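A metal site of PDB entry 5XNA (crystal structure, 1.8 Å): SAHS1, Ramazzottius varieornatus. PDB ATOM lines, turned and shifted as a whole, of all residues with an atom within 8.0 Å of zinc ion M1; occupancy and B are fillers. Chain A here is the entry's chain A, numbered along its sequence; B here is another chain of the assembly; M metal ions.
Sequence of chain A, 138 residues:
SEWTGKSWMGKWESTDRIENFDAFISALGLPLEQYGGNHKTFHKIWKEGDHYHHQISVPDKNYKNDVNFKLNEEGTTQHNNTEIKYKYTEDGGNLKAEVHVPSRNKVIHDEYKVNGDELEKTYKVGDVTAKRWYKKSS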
ATOM      1  N   ALA A  97      15.825  21.684  14.146  1.00  0.00           N
ATOM      2  CA  ALA A  97      16.088  20.509  14.957  1.00  0.00           C
ATOM      3  C   ALA A  97      14.857  20.203  15.804  1.00  0.00           C
ATOM      4  O   ALA A  97      14.302  21.113  16.444  1.00  0.00           O
ATOM      5  CB  ALA A  97      17.311  20.704  15.854  1.00  0.00           C
ATOM      6  N   GLU A  98      14.446  18.944  15.795  1.00  0.00           N
ATOM      7  CA  GLU A  98      13.379  18.413  16.643  1.00  0.00           C
ATOM      8  C   GLU A  98      14.026  17.667  17.804  1.00  0.00           C
ATOM      9  O   GLU A  98      14.751  16.701  17.565  1.00  0.00           O
ATOM     10  CB  GLU A  98      12.471  17.479  15.847  1.00  0.00           C
ATOM     11  CG  GLU A  98      11.248  17.024  16.620  1.00  0.00           C
ATOM     12  CD  GLU A  98      10.097  18.020  16.505  1.00  0.00           C
ATOM     13  OE1 GLU A  98      10.203  18.962  15.690  1.00  0.00           O
ATOM     14  OE2 GLU A  98       9.114  17.843  17.235  1.00  0.00           O
ATOM     15  N   VAL A  99      13.800  18.119  19.034  1.00  0.00           N
ATOM     16  CA  VAL A  99      14.531  17.587  20.186  1.00  0.00           C
ATOM     17  C   VAL A  99      13.546  16.992  21.187  1.00  0.00           C
ATOM     18  O   VAL A  99      12.611  17.669  21.619  1.00  0.00           O
ATOM     19  CB  VAL A  99      15.387  18.677  20.850  1.00  0.00           C
ATOM     20  CG1 VAL A  99      16.129  18.106  22.061  1.00  0.00           C
ATOM     21  CG2 VAL A  99      16.357  19.273  19.841  1.00  0.00           C
ATOM     22  N   HIS A 100      13.755  15.727  21.546  1.00  0.00           N
ATOM     23  CA  HIS A 100      12.997  15.087  22.627  1.00  0.00           C
ATOM     24  C   HIS A 100      13.841  15.054  23.889  1.00  0.00           C
ATOM     25  O   HIS A 100      15.013  14.670  23.854  1.00  0.00           O
ATOM     26  CB  HIS A 100      12.602  13.648  22.272  1.00  0.00           C
ATOM     27  CG  HIS A 100      11.466  13.511  21.288  1.00  0.00           C
ATOM     28  ND1 HIS A 100      11.627  13.694  19.930  1.00  0.00           N
ATOM     29  CD2 HIS A 100      10.181  13.133  21.473  1.00  0.00           C
ATOM     30  CE1 HIS A 100      10.480  13.453  19.320  1.00  0.00           C
ATOM     31  NE2 HIS A 100       9.584  13.115  20.237  1.00  0.00           N
ATOM     32  N   VAL A 107       9.342  18.498  24.400  1.00  0.00           N
ATOM     33  CA  VAL A 107       9.717  18.561  22.985  1.00  0.00           C
ATOM     34  C   VAL A 107      10.153  19.991  22.679  1.00  0.00           C
ATOM     35  O   VAL A 107       9.390  20.939  22.913  1.00  0.00           O
ATOM     36  CB  VAL A 107       8.569  18.131  22.067  1.00  0.00           C
ATOM     37  CG1 VAL A 107       8.978  18.316  20.599  1.00  0.00           C
ATOM     38  CG2 VAL A 107       8.143  16.691  22.345  1.00  0.00           C
ATOM     39  N   ILE A 108      11.369  20.148  22.164  1.00  0.00           N
ATOM     40  CA  ILE A 108      11.947  21.465  21.887  1.00  0.00           C
ATOM     41  C   ILE A 108      12.128  21.605  20.383  1.00  0.00           C
ATOM     42  O   ILE A 108      12.597  20.665  19.729  1.00  0.00           O
ATOM     43  CB  ILE A 108      13.306  21.655  22.592  1.00  0.00           C
ATOM     44  CG1 ILE A 108      13.175  21.540  24.103  1.00  0.00           C
ATOM     45  CG2 ILE A 108      13.943  22.977  22.172  1.00  0.00           C
ATOM     46  CD1 ILE A 108      14.500  21.406  24.809  1.00  0.00           C
ATOM     47  N   HIS A 109      11.703  22.735  19.839  1.00  0.00           N
ATOM     48  CA  HIS A 109      12.019  23.104  18.465  1.00  0.00           C
ATOM     49  C   HIS A 109      13.172  24.097  18.454  1.00  0.00           C
ATOM     50  O   HIS A 109      13.134  25.098  19.177  1.00  0.00           O
ATOM     51  CB  HIS A 109      10.810  23.735  17.752  1.00  0.00           C
ATOM     52  CG  HIS A 109       9.716  22.768  17.442  1.00  0.00           C
ATOM     53  ND1 HIS A 109       8.494  23.169  16.956  1.00  0.00           N
ATOM     54  CD2 HIS A 109       9.665  21.420  17.527  1.00  0.00           C
ATOM     55  CE1 HIS A 109       7.720  22.106  16.772  1.00  0.00           C
ATOM     56  NE2 HIS A 109       8.405  21.027  17.121  1.00  0.00           N
ATOM     57  N   ASP A 110      14.190  23.823  17.638  1.00  0.00           N
ATOM     58  CA  ASP A 110      15.232  24.782  17.306  1.00  0.00           C
ATOM     59  C   ASP A 110      15.100  25.146  15.836  1.00  0.00           C
ATOM     60  O   ASP A 110      14.799  24.274  15.008  1.00  0.00           O
ATOM     61  CB  ASP A 110      16.629  24.212  17.530  1.00  0.00           C
ATOM     62  CG  ASP A 110      16.910  23.883  18.955  1.00  0.00           C
ATOM     63  OD1 ASP A 110      16.369  24.584  19.832  1.00  0.00           O
ATOM     64  OD2 ASP A 110      17.669  22.925  19.195  1.00  0.00           O
ATOM     65  N   LYS A 124      11.691  26.979  20.840  1.00  0.00           N
ATOM     66  CA  LYS A 124      10.266  26.904  21.134  1.00  0.00           C
ATOM     67  C   LYS A 124       9.937  25.623  21.872  1.00  0.00           C
ATOM     68  O   LYS A 124      10.284  24.530  21.427  1.00  0.00           O
ATOM     69  CB  LYS A 124       9.439  26.991  19.847  1.00  0.00           C
ATOM     70  CG  LYS A 124       7.959  27.198  20.073  1.00  0.00           C
ATOM     71  CD  LYS A 124       7.231  27.353  18.746  1.00  0.00           C
ATOM     72  CE  LYS A 124       7.939  28.352  17.839  1.00  0.00           C
ATOM     73  NZ  LYS A 124       7.270  28.488  16.502  1.00  0.00           N
ATOM     74  N   ALA B  97      -0.942  22.103  15.418  1.00  0.00           N
ATOM     75  CA  ALA B  97      -1.029  20.871  16.193  1.00  0.00           C
ATOM     76  C   ALA B  97       0.317  20.154  16.138  1.00  0.00           C
ATOM     77  O   ALA B  97       0.887  19.974  15.052  1.00  0.00           O
ATOM     78  CB  ALA B  97      -2.137  19.952  15.663  1.00  0.00           C
ATOM     79  N   GLU B  98       0.844  19.815  17.300  1.00  0.00           N
ATOM     80  CA  GLU B  98       2.069  19.038  17.457  1.00  0.00           C
ATOM     81  C   GLU B  98       1.629  17.611  17.725  1.00  0.00           C
ATOM     82  O   GLU B  98       0.992  17.348  18.740  1.00  0.00           O
ATOM     83  CB  GLU B  98       2.879  19.582  18.626  1.00  0.00           C
ATOM     84  CG  GLU B  98       4.182  18.852  18.900  1.00  0.00           C
ATOM     85  CD  GLU B  98       5.279  19.289  17.967  1.00  0.00           C
ATOM     86  OE1 GLU B  98       5.134  20.347  17.303  1.00  0.00           O
ATOM     87  OE2 GLU B  98       6.287  18.565  17.891  1.00  0.00           O
ATOM     88  N   VAL B  99       1.903  16.697  16.792  1.00  0.00           N
ATOM     89  CA  VAL B  99       1.285  15.366  16.855  1.00  0.00           C
ATOM     90  C   VAL B  99       2.410  14.342  16.868  1.00  0.00           C
ATOM     91  O   VAL B  99       3.188  14.265  15.908  1.00  0.00           O
ATOM     92  CB  VAL B  99       0.339  15.135  15.676  1.00  0.00           C
ATOM     93  CG1 VAL B  99      -0.255  13.745  15.732  1.00  0.00           C
ATOM     94  CG2 VAL B  99      -0.766  16.229  15.667  1.00  0.00           C
ATOM     95  N   HIS B 100       2.498  13.571  17.936  1.00  0.00           N
ATOM     96  CA  HIS B 100       3.549  12.577  18.073  1.00  0.00           C
ATOM     97  C   HIS B 100       2.936  11.188  18.137  1.00  0.00           C
ATOM     98  O   HIS B 100       1.930  10.960  18.826  1.00  0.00           O
ATOM     99  CB  HIS B 100       4.418  12.851  19.292  1.00  0.00           C
ATOM    100  CG  HIS B 100       5.290  14.067  19.161  1.00  0.00           C
ATOM    101  ND1 HIS B 100       6.633  14.050  19.404  1.00  0.00           N
ATOM    102  CD2 HIS B 100       4.985  15.337  18.781  1.00  0.00           C
ATOM    103  CE1 HIS B 100       7.144  15.256  19.200  1.00  0.00           C
ATOM    104  NE2 HIS B 100       6.156  16.055  18.830  1.00  0.00           N
ATOM    105  N   VAL B 107       6.717  12.238  13.988  1.00  0.00           N
ATOM    106  CA  VAL B 107       6.302  13.550  14.451  1.00  0.00           C
ATOM    107  C   VAL B 107       5.641  14.261  13.291  1.00  0.00           C
ATOM    108  O   VAL B 107       6.254  14.414  12.222  1.00  0.00           O
ATOM    109  CB  VAL B 107       7.486  14.385  14.976  1.00  0.00           C
ATOM    110  CG1 VAL B 107       6.981  15.789  15.359  1.00  0.00           C
ATOM    111  CG2 VAL B 107       8.150  13.711  16.157  1.00  0.00           C
ATOM    112  N   ILE B 108       4.421  14.733  13.496  1.00  0.00           N
ATOM    113  CA  ILE B 108       3.677  15.455  12.472  1.00  0.00           C
ATOM    114  C   ILE B 108       3.471  16.877  12.985  1.00  0.00           C
ATOM    115  O   ILE B 108       3.075  17.057  14.142  1.00  0.00           O
ATOM    116  CB  ILE B 108       2.319  14.779  12.187  1.00  0.00           C
ATOM    117  CG1 ILE B 108       2.534  13.339  11.725  1.00  0.00           C
ATOM    118  CG2 ILE B 108       1.499  15.637  11.205  1.00  0.00           C
ATOM    119  CD1 ILE B 108       1.340  12.445  11.943  1.00  0.00           C
ATOM    120  N   HIS B 109       3.756  17.854  12.143  1.00  0.00           N
ATOM    121  CA  HIS B 109       3.456  19.264  12.420  1.00  0.00           C
ATOM    122  C   HIS B 109       2.315  19.709  11.508  1.00  0.00           C
ATOM    123  O   HIS B 109       2.495  19.781  10.295  1.00  0.00           O
ATOM    124  CB  HIS B 109       4.675  20.162  12.182  1.00  0.00           C
ATOM    125  CG  HIS B 109       5.795  19.928  13.146  1.00  0.00           C
ATOM    126  ND1 HIS B 109       7.090  20.313  12.879  1.00  0.00           N
ATOM    127  CD2 HIS B 109       5.814  19.397  14.396  1.00  0.00           C
ATOM    128  CE1 HIS B 109       7.863  19.988  13.900  1.00  0.00           C
ATOM    129  NE2 HIS B 109       7.115  19.435  14.833  1.00  0.00           N
HETATM  130 ZN    ZN M   1       7.737  19.256  16.726  1.00  0.00          ZN
HETATM  131 ZN    ZN M   2       7.747  12.371  20.004  1.00  0.00          ZN
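Val 107 of chain B touches zinc ion M1 (CG1 to ZN, 3.8 Å).
Along chain A the residues within 4 Å of zinc ion M1 span positions 98 to 109.
The backbone carbonyl oxygen (O) of Lys 124 lies within hydrogen-bond range of the backbone NH (N) of His 109 of chain A.
The side-chain carboxylate (OE2) of Glu 98 of chain B sits close to a ring nitrogen (NE2) of His 100 of chain B.
Zinc ion M1 is bound by a ring nitrogen (NE2) of His 109 of chain A (1.9 Å), the side-chain carboxylate (OE2) of Glu 98 of chain B (2.0 Å), a ring nitrogen (NE2) of His 109 of chain B (2.0 Å) and the side-chain carboxylate (OE2) of Glu 98 of chain A (2.0 Å).
Zinc ion M1 has four donor atoms within binding distance.
Slightly farther from zinc ion M1 lies the side-chain carboxylate (OE1) of Glu 98 of chain A (2.7 Å).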
